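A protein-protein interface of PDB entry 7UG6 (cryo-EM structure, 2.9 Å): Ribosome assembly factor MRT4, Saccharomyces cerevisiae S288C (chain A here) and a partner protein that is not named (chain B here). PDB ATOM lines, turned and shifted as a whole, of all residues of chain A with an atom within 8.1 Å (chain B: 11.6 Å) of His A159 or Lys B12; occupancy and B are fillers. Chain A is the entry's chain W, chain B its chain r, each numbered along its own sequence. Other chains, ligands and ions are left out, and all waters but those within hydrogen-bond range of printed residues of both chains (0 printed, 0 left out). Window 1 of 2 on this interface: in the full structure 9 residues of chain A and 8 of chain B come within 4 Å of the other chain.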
ATOM      1  N   VAL A 142      18.074 -15.640  -4.254  1.00  0.00           N
ATOM      2  CA  VAL A 142      17.867 -17.038  -4.589  1.00  0.00           C
ATOM      3  C   VAL A 142      18.878 -17.430  -5.654  1.00  0.00           C
ATOM      4  O   VAL A 142      19.103 -16.704  -6.627  1.00  0.00           O
ATOM      5  CB  VAL A 142      16.415 -17.297  -5.029  1.00  0.00           C
ATOM      6  CG1 VAL A 142      15.469 -16.882  -3.936  1.00  0.00           C
ATOM      7  CG2 VAL A 142      16.074 -16.584  -6.298  1.00  0.00           C
ATOM      8  N   PRO A 156      23.644 -17.019  -9.014  1.00  0.00           N
ATOM      9  CA  PRO A 156      22.317 -16.445  -8.778  1.00  0.00           C
ATOM     10  C   PRO A 156      21.354 -16.828  -9.882  1.00  0.00           C
ATOM     11  O   PRO A 156      21.745 -17.000 -11.037  1.00  0.00           O
ATOM     12  CB  PRO A 156      22.581 -14.938  -8.761  1.00  0.00           C
ATOM     13  CG  PRO A 156      24.010 -14.809  -8.477  1.00  0.00           C
ATOM     14  CD  PRO A 156      24.659 -15.967  -9.150  1.00  0.00           C
ATOM     15  N   MET A 157      20.086 -16.973  -9.516  1.00  0.00           N
ATOM     16  CA  MET A 157      19.077 -17.302 -10.503  1.00  0.00           C
ATOM     17  C   MET A 157      18.935 -16.160 -11.492  1.00  0.00           C
ATOM     18  O   MET A 157      19.017 -14.988 -11.125  1.00  0.00           O
ATOM     19  CB  MET A 157      17.741 -17.596  -9.833  1.00  0.00           C
ATOM     20  CG  MET A 157      16.680 -18.064 -10.807  1.00  0.00           C
ATOM     21  SD  MET A 157      15.094 -18.433 -10.062  1.00  0.00           S
ATOM     22  CE  MET A 157      15.492 -19.944  -9.212  1.00  0.00           C
ATOM     23  N   ILE A 158      18.748 -16.517 -12.760  1.00  0.00           N
ATOM     24  CA  ILE A 158      18.623 -15.535 -13.826  1.00  0.00           C
ATOM     25  C   ILE A 158      17.482 -14.584 -13.510  1.00  0.00           C
ATOM     26  O   ILE A 158      16.378 -15.011 -13.155  1.00  0.00           O
ATOM     27  CB  ILE A 158      18.390 -16.235 -15.175  1.00  0.00           C
ATOM     28  CG1 ILE A 158      19.483 -17.261 -15.466  1.00  0.00           C
ATOM     29  CG2 ILE A 158      18.351 -15.225 -16.292  1.00  0.00           C
ATOM     30  CD1 ILE A 158      19.175 -18.663 -15.010  1.00  0.00           C
ATOM     31  N   HIS A 159      17.746 -13.288 -13.646  1.00  0.00           N
ATOM     32  CA  HIS A 159      16.714 -12.284 -13.432  1.00  0.00           C
ATOM     33  C   HIS A 159      15.516 -12.509 -14.330  1.00  0.00           C
ATOM     34  O   HIS A 159      14.396 -12.138 -13.975  1.00  0.00           O
ATOM     35  CB  HIS A 159      17.291 -10.912 -13.710  1.00  0.00           C
ATOM     36  CG  HIS A 159      17.928 -10.813 -15.055  1.00  0.00           C
ATOM     37  ND1 HIS A 159      19.246 -11.138 -15.277  1.00  0.00           N
ATOM     38  CD2 HIS A 159      17.428 -10.432 -16.251  1.00  0.00           C
ATOM     39  CE1 HIS A 159      19.532 -10.961 -16.552  1.00  0.00           C
ATOM     40  NE2 HIS A 159      18.447 -10.529 -17.165  1.00  0.00           N
ATOM     41  N   SER A 160      15.728 -13.099 -15.503  1.00  0.00           N
ATOM     42  CA  SER A 160      14.627 -13.335 -16.420  1.00  0.00           C
ATOM     43  C   SER A 160      13.702 -14.433 -15.941  1.00  0.00           C
ATOM     44  O   SER A 160      12.632 -14.612 -16.527  1.00  0.00           O
ATOM     45  CB  SER A 160      15.160 -13.684 -17.802  1.00  0.00           C
ATOM     46  OG  SER A 160      15.486 -15.056 -17.870  1.00  0.00           O
ATOM     47  N   LEU A 161      14.086 -15.180 -14.914  1.00  0.00           N
ATOM     48  CA  LEU A 161      13.213 -16.186 -14.337  1.00  0.00           C
ATOM     49  C   LEU A 161      12.277 -15.617 -13.290  1.00  0.00           C
ATOM     50  O   LEU A 161      11.363 -16.319 -12.852  1.00  0.00           O
ATOM     51  CB  LEU A 161      14.034 -17.313 -13.725  1.00  0.00           C
ATOM     52  CG  LEU A 161      14.453 -18.350 -14.752  1.00  0.00           C
ATOM     53  CD1 LEU A 161      15.591 -19.187 -14.222  1.00  0.00           C
ATOM     54  CD2 LEU A 161      13.266 -19.201 -15.131  1.00  0.00           C
ATOM     55  N   GLU A 162      12.479 -14.373 -12.882  1.00  0.00           N
ATOM     56  CA  GLU A 162      11.660 -13.804 -11.820  1.00  0.00           C
ATOM     57  C   GLU A 162      10.184 -13.697 -12.176  1.00  0.00           C
ATOM     58  O   GLU A 162       9.357 -13.928 -11.279  1.00  0.00           O
ATOM     59  CB  GLU A 162      12.236 -12.450 -11.396  1.00  0.00           C
ATOM     60  CG  GLU A 162      11.613 -11.879 -10.138  1.00  0.00           C
ATOM     61  CD  GLU A 162      10.336 -11.134 -10.393  1.00  0.00           C
ATOM     62  OE1 GLU A 162      10.182 -10.584 -11.496  1.00  0.00           O
ATOM     63  OE2 GLU A 162       9.472 -11.111  -9.499  1.00  0.00           O
ATOM     64  N   PRO A 163       9.775 -13.309 -13.389  1.00  0.00           N
ATOM     65  CA  PRO A 163       8.338 -13.327 -13.679  1.00  0.00           C
ATOM     66  C   PRO A 163       7.707 -14.695 -13.505  1.00  0.00           C
ATOM     67  O   PRO A 163       6.570 -14.784 -13.038  1.00  0.00           O
ATOM     68  CB  PRO A 163       8.279 -12.844 -15.128  1.00  0.00           C
ATOM     69  CG  PRO A 163       9.442 -11.992 -15.261  1.00  0.00           C
ATOM     70  CD  PRO A 163      10.512 -12.657 -14.483  1.00  0.00           C
ATOM     71  N   THR A 164       8.416 -15.769 -13.844  1.00  0.00           N
ATOM     72  CA  THR A 164       7.886 -17.105 -13.603  1.00  0.00           C
ATOM     73  C   THR A 164       7.816 -17.410 -12.115  1.00  0.00           C
ATOM     74  O   THR A 164       6.824 -17.961 -11.632  1.00  0.00           O
ATOM     75  CB  THR A 164       8.741 -18.136 -14.321  1.00  0.00           C
ATOM     76  OG1 THR A 164      10.061 -18.105 -13.776  1.00  0.00           O
ATOM     77  CG2 THR A 164       8.814 -17.807 -15.787  1.00  0.00           C
ATOM     78  N   MET A 165       8.859 -17.037 -11.370  1.00  0.00           N
ATOM     79  CA  MET A 165       8.864 -17.245  -9.926  1.00  0.00           C
ATOM     80  C   MET A 165       7.733 -16.494  -9.245  1.00  0.00           C
ATOM     81  O   MET A 165       7.221 -16.944  -8.217  1.00  0.00           O
ATOM     82  CB  MET A 165      10.198 -16.800  -9.327  1.00  0.00           C
ATOM     83  CG  MET A 165      11.394 -17.560  -9.822  1.00  0.00           C
ATOM     84  SD  MET A 165      11.664 -19.087  -8.926  1.00  0.00           S
ATOM     85  CE  MET A 165      12.119 -18.449  -7.322  1.00  0.00           C
ATOM     86  N   ARG A 166       7.331 -15.358  -9.798  1.00  0.00           N
ATOM     87  CA  ARG A 166       6.332 -14.510  -9.172  1.00  0.00           C
ATOM     88  C   ARG A 166       4.919 -14.798  -9.659  1.00  0.00           C
ATOM     89  O   ARG A 166       3.956 -14.556  -8.930  1.00  0.00           O
ATOM     90  CB  ARG A 166       6.676 -13.048  -9.429  1.00  0.00           C
ATOM     91  CG  ARG A 166       5.959 -12.087  -8.540  1.00  0.00           C
ATOM     92  CD  ARG A 166       6.245 -10.680  -8.960  1.00  0.00           C
ATOM     93  NE  ARG A 166       5.605 -10.368 -10.227  1.00  0.00           N
ATOM     94  CZ  ARG A 166       6.270 -10.108 -11.341  1.00  0.00           C
ATOM     95  NH1 ARG A 166       7.587 -10.122 -11.334  1.00  0.00           N
ATOM     96  NH2 ARG A 166       5.620  -9.829 -12.454  1.00  0.00           N
ATOM     97  N   LYS A 174      11.379 -10.509  -5.339  1.00  0.00           N
ATOM     98  CA  LYS A 174      11.743  -9.136  -5.647  1.00  0.00           C
ATOM     99  C   LYS A 174      12.967  -9.162  -6.544  1.00  0.00           C
ATOM    100  O   LYS A 174      13.662 -10.174  -6.635  1.00  0.00           O
ATOM    101  CB  LYS A 174      12.078  -8.318  -4.390  1.00  0.00           C
ATOM    102  CG  LYS A 174      10.899  -7.735  -3.636  1.00  0.00           C
ATOM    103  CD  LYS A 174      10.145  -8.807  -2.875  1.00  0.00           C
ATOM    104  CE  LYS A 174      10.968  -9.342  -1.713  1.00  0.00           C
ATOM    105  NZ  LYS A 174      10.208 -10.353  -0.924  1.00  0.00           N
ATOM    106  N   ILE A 175      13.231  -8.042  -7.200  1.00  0.00           N
ATOM    107  CA  ILE A 175      14.478  -7.838  -7.920  1.00  0.00           C
ATOM    108  C   ILE A 175      15.253  -6.754  -7.194  1.00  0.00           C
ATOM    109  O   ILE A 175      14.834  -5.593  -7.167  1.00  0.00           O
ATOM    110  CB  ILE A 175      14.229  -7.445  -9.380  1.00  0.00           C
ATOM    111  CG1 ILE A 175      13.534  -8.567 -10.139  1.00  0.00           C
ATOM    112  CG2 ILE A 175      15.536  -7.087 -10.043  1.00  0.00           C
ATOM    113  CD1 ILE A 175      14.470  -9.632 -10.621  1.00  0.00           C
ATOM    114  N   LYS A 176      16.374  -7.120  -6.598  1.00  0.00           N
ATOM    115  CA  LYS A 176      17.230  -6.173  -5.901  1.00  0.00           C
ATOM    116  C   LYS A 176      18.569  -6.180  -6.615  1.00  0.00           C
ATOM    117  O   LYS A 176      19.354  -7.118  -6.449  1.00  0.00           O
ATOM    118  CB  LYS A 176      17.395  -6.547  -4.432  1.00  0.00           C
ATOM    119  CG  LYS A 176      16.100  -6.802  -3.691  1.00  0.00           C
ATOM    120  CD  LYS A 176      15.469  -5.528  -3.179  1.00  0.00           C
ATOM    121  CE  LYS A 176      14.284  -5.841  -2.274  1.00  0.00           C
ATOM    122  NZ  LYS A 176      13.732  -4.628  -1.612  1.00  0.00           N
ATOM    123  N   ALA A 177      18.822  -5.136  -7.402  1.00  0.00           N
ATOM    124  CA  ALA A 177      20.044  -5.011  -8.195  1.00  0.00           C
ATOM    125  C   ALA A 177      20.216  -6.195  -9.137  1.00  0.00           C
ATOM    126  O   ALA A 177      21.311  -6.730  -9.300  1.00  0.00           O
ATOM    127  CB  ALA A 177      21.276  -4.837  -7.305  1.00  0.00           C
ATOM    128  N   GLY A 178      19.124  -6.606  -9.764  1.00  0.00           N
ATOM    129  CA  GLY A 178      19.199  -7.614 -10.793  1.00  0.00           C
ATOM    130  C   GLY A 178      19.205  -9.030 -10.299  1.00  0.00           C
ATOM    131  O   GLY A 178      19.428  -9.948 -11.088  1.00  0.00           O
ATOM    132  N   LYS A 179      18.962  -9.243  -9.015  1.00  0.00           N
ATOM    133  CA  LYS A 179      18.977 -10.572  -8.429  1.00  0.00           C
ATOM    134  C   LYS A 179      17.620 -10.862  -7.822  1.00  0.00           C
ATOM    135  O   LYS A 179      17.096 -10.048  -7.060  1.00  0.00           O
ATOM    136  CB  LYS A 179      20.063 -10.676  -7.370  1.00  0.00           C
ATOM    137  CG  LYS A 179      21.439 -10.635  -7.954  1.00  0.00           C
ATOM    138  CD  LYS A 179      22.465 -10.396  -6.899  1.00  0.00           C
ATOM    139  CE  LYS A 179      23.836 -10.467  -7.507  1.00  0.00           C
ATOM    140  NZ  LYS A 179      24.030  -9.397  -8.510  1.00  0.00           N
ATOM    141  N   ILE A 180      17.048 -12.010  -8.170  1.00  0.00           N
ATOM    142  CA  ILE A 180      15.790 -12.417  -7.567  1.00  0.00           C
ATOM    143  C   ILE A 180      16.004 -12.602  -6.078  1.00  0.00           C
ATOM    144  O   ILE A 180      17.024 -13.146  -5.645  1.00  0.00           O
ATOM    145  CB  ILE A 180      15.275 -13.708  -8.219  1.00  0.00           C
ATOM    146  CG1 ILE A 180      15.367 -13.620  -9.729  1.00  0.00           C
ATOM    147  CG2 ILE A 180      13.847 -13.976  -7.817  1.00  0.00           C
ATOM    148  CD1 ILE A 180      14.840 -14.830 -10.389  1.00  0.00           C
ATOM    149  N   ASN B   4      24.383   4.169 -21.931  1.00  0.00           N
ATOM    150  CA  ASN B   4      24.627   3.081 -22.872  1.00  0.00           C
ATOM    151  C   ASN B   4      23.632   1.968 -22.623  1.00  0.00           C
ATOM    152  O   ASN B   4      23.810   1.201 -21.672  1.00  0.00           O
ATOM    153  CB  ASN B   4      26.047   2.547 -22.734  1.00  0.00           C
ATOM    154  CG  ASN B   4      27.058   3.398 -23.432  1.00  0.00           C
ATOM    155  OD1 ASN B   4      26.913   3.719 -24.603  1.00  0.00           O
ATOM    156  ND2 ASN B   4      28.110   3.748 -22.726  1.00  0.00           N
ATOM    157  N   ASP B   5      22.628   1.849 -23.492  1.00  0.00           N
ATOM    158  CA  ASP B   5      21.628   0.795 -23.364  1.00  0.00           C
ATOM    159  C   ASP B   5      21.031   0.804 -21.968  1.00  0.00           C
ATOM    160  O   ASP B   5      20.879  -0.234 -21.332  1.00  0.00           O
ATOM    161  CB  ASP B   5      22.223  -0.576 -23.681  1.00  0.00           C
ATOM    162  CG  ASP B   5      22.578  -0.740 -25.143  1.00  0.00           C
ATOM    163  OD1 ASP B   5      21.918  -0.108 -25.993  1.00  0.00           O
ATOM    164  OD2 ASP B   5      23.518  -1.507 -25.445  1.00  0.00           O
ATOM    165  N   TYR B   6      20.746   2.000 -21.463  1.00  0.00           N
ATOM    166  CA  TYR B   6      20.352   2.124 -20.073  1.00  0.00           C
ATOM    167  C   TYR B   6      18.967   1.570 -19.810  1.00  0.00           C
ATOM    168  O   TYR B   6      18.603   1.384 -18.648  1.00  0.00           O
ATOM    169  CB  TYR B   6      20.442   3.577 -19.622  1.00  0.00           C
ATOM    170  CG  TYR B   6      19.907   4.600 -20.583  1.00  0.00           C
ATOM    171  CD1 TYR B   6      20.712   5.144 -21.560  1.00  0.00           C
ATOM    172  CD2 TYR B   6      18.618   5.076 -20.467  1.00  0.00           C
ATOM    173  CE1 TYR B   6      20.237   6.091 -22.418  1.00  0.00           C
ATOM    174  CE2 TYR B   6      18.138   6.019 -21.325  1.00  0.00           C
ATOM    175  CZ  TYR B   6      18.948   6.521 -22.294  1.00  0.00           C
ATOM    176  OH  TYR B   6      18.465   7.472 -23.147  1.00  0.00           O
ATOM    177  N   ILE B   7      18.208   1.238 -20.847  1.00  0.00           N
ATOM    178  CA  ILE B   7      16.929   0.604 -20.594  1.00  0.00           C
ATOM    179  C   ILE B   7      17.075  -0.910 -20.494  1.00  0.00           C
ATOM    180  O   ILE B   7      16.420  -1.525 -19.661  1.00  0.00           O
ATOM    181  CB  ILE B   7      15.891   1.028 -21.638  1.00  0.00           C
ATOM    182  CG1 ILE B   7      15.558   2.500 -21.450  1.00  0.00           C
ATOM    183  CG2 ILE B   7      14.620   0.245 -21.466  1.00  0.00           C
ATOM    184  CD1 ILE B   7      14.980   2.813 -20.113  1.00  0.00           C
ATOM    185  N   GLU B   8      17.945  -1.554 -21.285  1.00  0.00           N
ATOM    186  CA  GLU B   8      18.260  -2.939 -20.929  1.00  0.00           C
ATOM    187  C   GLU B   8      18.872  -3.017 -19.546  1.00  0.00           C
ATOM    188  O   GLU B   8      18.582  -3.945 -18.791  1.00  0.00           O
ATOM    189  CB  GLU B   8      19.214  -3.650 -21.890  1.00  0.00           C
ATOM    190  CG  GLU B   8      18.743  -4.032 -23.261  1.00  0.00           C
ATOM    191  CD  GLU B   8      18.898  -2.940 -24.227  1.00  0.00           C
ATOM    192  OE1 GLU B   8      19.431  -1.895 -23.815  1.00  0.00           O
ATOM    193  OE2 GLU B   8      18.540  -3.137 -25.407  1.00  0.00           O
ATOM    194  N   ARG B   9      19.747  -2.081 -19.206  1.00  0.00           N
ATOM    195  CA  ARG B   9      20.305  -2.091 -17.867  1.00  0.00           C
ATOM    196  C   ARG B   9      19.211  -1.920 -16.832  1.00  0.00           C
ATOM    197  O   ARG B   9      19.237  -2.568 -15.784  1.00  0.00           O
ATOM    198  CB  ARG B   9      21.364  -1.008 -17.725  1.00  0.00           C
ATOM    199  CG  ARG B   9      22.727  -1.438 -18.207  1.00  0.00           C
ATOM    200  CD  ARG B   9      23.444  -0.295 -18.878  1.00  0.00           C
ATOM    201  NE  ARG B   9      23.735   0.771 -17.930  1.00  0.00           N
ATOM    202  CZ  ARG B   9      23.845   2.049 -18.258  1.00  0.00           C
ATOM    203  NH1 ARG B   9      23.683   2.422 -19.513  1.00  0.00           N
ATOM    204  NH2 ARG B   9      24.108   2.956 -17.331  1.00  0.00           N
ATOM    205  N   HIS B  10      18.220  -1.082 -17.116  1.00  0.00           N
ATOM    206  CA  HIS B  10      17.137  -0.920 -16.158  1.00  0.00           C
ATOM    207  C   HIS B  10      16.282  -2.176 -16.048  1.00  0.00           C
ATOM    208  O   HIS B  10      15.888  -2.561 -14.945  1.00  0.00           O
ATOM    209  CB  HIS B  10      16.272   0.270 -16.524  1.00  0.00           C
ATOM    210  CG  HIS B  10      15.210   0.545 -15.519  1.00  0.00           C
ATOM    211  ND1 HIS B  10      15.478   1.119 -14.299  1.00  0.00           N
ATOM    212  CD2 HIS B  10      13.886   0.287 -15.530  1.00  0.00           C
ATOM    213  CE1 HIS B  10      14.358   1.222 -13.611  1.00  0.00           C
ATOM    214  NE2 HIS B  10      13.377   0.725 -14.336  1.00  0.00           N
ATOM    215  N   ILE B  11      15.974  -2.822 -17.171  1.00  0.00           N
ATOM    216  CA  ILE B  11      15.200  -4.059 -17.127  1.00  0.00           C
ATOM    217  C   ILE B  11      15.969  -5.157 -16.413  1.00  0.00           C
ATOM    218  O   ILE B  11      15.386  -5.972 -15.694  1.00  0.00           O
ATOM    219  CB  ILE B  11      14.776  -4.505 -18.538  1.00  0.00           C
ATOM    220  CG1 ILE B  11      14.122  -3.372 -19.327  1.00  0.00           C
ATOM    221  CG2 ILE B  11      13.900  -5.726 -18.480  1.00  0.00           C
ATOM    222  CD1 ILE B  11      13.011  -2.658 -18.601  1.00  0.00           C
ATOM    223  N   LYS B  12      17.278  -5.216 -16.610  1.00  0.00           N
ATOM    224  CA  LYS B  12      18.066  -6.214 -15.906  1.00  0.00           C
ATOM    225  C   LYS B  12      18.097  -5.929 -14.415  1.00  0.00           C
ATOM    226  O   LYS B  12      17.850  -6.824 -13.604  1.00  0.00           O
ATOM    227  CB  LYS B  12      19.478  -6.264 -16.476  1.00  0.00           C
ATOM    228  CG  LYS B  12      19.708  -7.365 -17.492  1.00  0.00           C
ATOM    229  CD  LYS B  12      19.166  -6.992 -18.853  1.00  0.00           C
ATOM    230  CE  LYS B  12      19.584  -7.969 -19.927  1.00  0.00           C
ATOM    231  NZ  LYS B  12      19.096  -7.537 -21.263  1.00  0.00           N
ATOM    232  N   GLN B  13      18.360  -4.688 -14.033  1.00  0.00           N
ATOM    233  CA  GLN B  13      18.568  -4.352 -12.638  1.00  0.00           C
ATOM    234  C   GLN B  13      17.281  -4.261 -11.834  1.00  0.00           C
ATOM    235  O   GLN B  13      17.322  -4.442 -10.616  1.00  0.00           O
ATOM    236  CB  GLN B  13      19.318  -3.026 -12.530  1.00  0.00           C
ATOM    237  CG  GLN B  13      20.752  -3.096 -12.978  1.00  0.00           C
ATOM    238  CD  GLN B  13      21.617  -3.833 -12.003  1.00  0.00           C
ATOM    239  OE1 GLN B  13      21.448  -3.706 -10.797  1.00  0.00           O
ATOM    240  NE2 GLN B  13      22.550  -4.619 -12.514  1.00  0.00           N
ATOM    241  N   HIS B  14      16.148  -3.980 -12.468  1.00  0.00           N
ATOM    242  CA  HIS B  14      14.909  -3.755 -11.746  1.00  0.00           C
ATOM    243  C   HIS B  14      13.712  -4.487 -12.319  1.00  0.00           C
ATOM    244  O   HIS B  14      12.642  -4.438 -11.710  1.00  0.00           O
ATOM    245  CB  HIS B  14      14.584  -2.259 -11.699  1.00  0.00           C
ATOM    246  CG  HIS B  14      15.735  -1.409 -11.277  1.00  0.00           C
ATOM    247  ND1 HIS B  14      16.038  -1.171  -9.957  1.00  0.00           N
ATOM    248  CD2 HIS B  14      16.666  -0.749 -12.000  1.00  0.00           C
ATOM    249  CE1 HIS B  14      17.103  -0.395  -9.883  1.00  0.00           C
ATOM    250  NE2 HIS B  14      17.504  -0.126 -11.111  1.00  0.00           N
ATOM    251  N   GLY B  15      13.845  -5.154 -13.446  1.00  0.00           N
ATOM    252  CA  GLY B  15      12.724  -5.842 -14.026  1.00  0.00           C
ATOM    253  C   GLY B  15      11.791  -4.890 -14.742  1.00  0.00           C
ATOM    254  O   GLY B  15      12.056  -3.700 -14.903  1.00  0.00           O
ATOM    255  N   LYS B  16      10.682  -5.444 -15.194  1.00  0.00           N
ATOM    256  CA  LYS B  16       9.628  -4.676 -15.820  1.00  0.00           C
ATOM    257  C   LYS B  16       8.474  -4.547 -14.841  1.00  0.00           C
ATOM    258  O   LYS B  16       8.514  -5.095 -13.741  1.00  0.00           O
ATOM    259  CB  LYS B  16       9.211  -5.336 -17.127  1.00  0.00           C
ATOM    260  CG  LYS B  16      10.401  -5.691 -17.973  1.00  0.00           C
ATOM    261  CD  LYS B  16      10.010  -6.329 -19.270  1.00  0.00           C
ATOM    262  CE  LYS B  16       9.635  -5.276 -20.287  1.00  0.00           C
ATOM    263  NZ  LYS B  16      10.810  -4.504 -20.763  1.00  0.00           N
ATOM    264  N   ARG B  17       7.450  -3.803 -15.239  1.00  0.00           N
ATOM    265  CA  ARG B  17       6.311  -3.585 -14.360  1.00  0.00           C
ATOM    266  C   ARG B  17       5.628  -4.911 -14.066  1.00  0.00           C
ATOM    267  O   ARG B  17       5.647  -5.827 -14.887  1.00  0.00           O
ATOM    268  CB  ARG B  17       5.332  -2.601 -14.990  1.00  0.00           C
ATOM    269  CG  ARG B  17       5.797  -1.164 -14.932  1.00  0.00           C
ATOM    270  CD  ARG B  17       4.932  -0.264 -15.769  1.00  0.00           C
ATOM    271  NE  ARG B  17       3.536  -0.299 -15.362  1.00  0.00           N
ATOM    272  CZ  ARG B  17       2.989   0.562 -14.516  1.00  0.00           C
ATOM    273  NH1 ARG B  17       3.726   1.524 -13.987  1.00  0.00           N
ATOM    274  NH2 ARG B  17       1.711   0.468 -14.194  1.00  0.00           N
ATOM    275  N   LEU B  18       5.053  -5.023 -12.872  1.00  0.00           N
ATOM    276  CA  LEU B  18       4.678  -6.336 -12.367  1.00  0.00           C
ATOM    277  C   LEU B  18       3.614  -7.001 -13.223  1.00  0.00           C
ATOM    278  O   LEU B  18       3.539  -8.231 -13.263  1.00  0.00           O
ATOM    279  CB  LEU B  18       4.201  -6.226 -10.930  1.00  0.00           C
ATOM    280  CG  LEU B  18       5.251  -5.874  -9.893  1.00  0.00           C
ATOM    281  CD1 LEU B  18       4.634  -5.947  -8.534  1.00  0.00           C
ATOM    282  CD2 LEU B  18       6.388  -6.825  -9.978  1.00  0.00           C
ATOM    283  N   GLU B  21       3.884  -8.783 -18.256  1.00  0.00           N
ATOM    284  CA  GLU B  21       3.645 -10.006 -19.010  1.00  0.00           C
ATOM    285  C   GLU B  21       2.163 -10.197 -19.279  1.00  0.00           C
ATOM    286  O   GLU B  21       1.756 -10.455 -20.413  1.00  0.00           O
ATOM    287  CB  GLU B  21       4.205 -11.208 -18.257  1.00  0.00           C
ATOM    288  CG  GLU B  21       5.573 -10.993 -17.657  1.00  0.00           C
ATOM    289  CD  GLU B  21       6.560 -10.451 -18.656  1.00  0.00           C
ATOM    290  OE1 GLU B  21       6.902 -11.182 -19.607  1.00  0.00           O
ATOM    291  OE2 GLU B  21       7.002  -9.299 -18.487  1.00  0.00           O
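The backbone carbonyl oxygen (O) of Gln B13 sits at hydrogen-bond distance from the backbone NH (N) of Gly A178 (2.9 Å).
The side-chain amide oxygen (OE1) of Gln B13 sits close to the backbone carbonyl oxygen (O) of Ala A177 (3.4 Å).
The guanidinium group (NH2) of Arg A166 lies within hydrogen-bond range of the backbone carbonyl oxygen (O) of Leu B18, at 2.7 Å.
Hydrophobic or aromatic side chains of chain B that line the printed part of chain A: Leu B18.
Among the printed residues, no Asp or Glu carboxylate lies within 4 Å of a Lys or Arg side-chain nitrogen of the other chain.
Among the printed residues, merely in contact across the chains: Gly A178 with Lys B12 (3.2 Å), Ile A175 with Gln B13 (3.2 Å), His A159 with Lys B12 (3.4 Å) and Ile A175 with His B14 (3.8 Å).
OE1 of Glu A162 is in salt-bridge range of NH1 of Arg A166, at 2.6 Å.
Of chain B, only Lys B12 (3.4 Å) comes within 4 Å of His A159.
Lys B12 touches just these residues of chain A: His A159 (3.4 Å) and Gly A178 (3.2 Å).
No residue of chain B comes within 4 Å of Ile A158.
No residue of chain B comes within 4 Å of Ser A160.
No residue of chain B comes within 4 Å of Leu A161.
No residue of chain B comes within 4 Å of Glu A162.
Of chain B, only Gln B13 (3.2 Å) comes within 4 Å of Ala A177.
Of the printed residues of chain A, Leu B18 touches Arg A166 (2.7 Å).
Printed residues of chain B within 4 Å of Arg A166: Leu B18 (2.7 Å).
Printed residues of chain A within 4 Å of Gln B13: Ile A175, Ala A177 and Gly A178.
Printed residues of chain B within 4 Å of Ile A175: Gln B13 (3.2 Å) and His B14 (3.8 Å).
The nearest residue of chain B that does not touch His A159 is Ile B11 (4.9 Å).
The nearest printed residue of chain B that does not touch Arg A166 is Arg B17 (4.7 Å).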
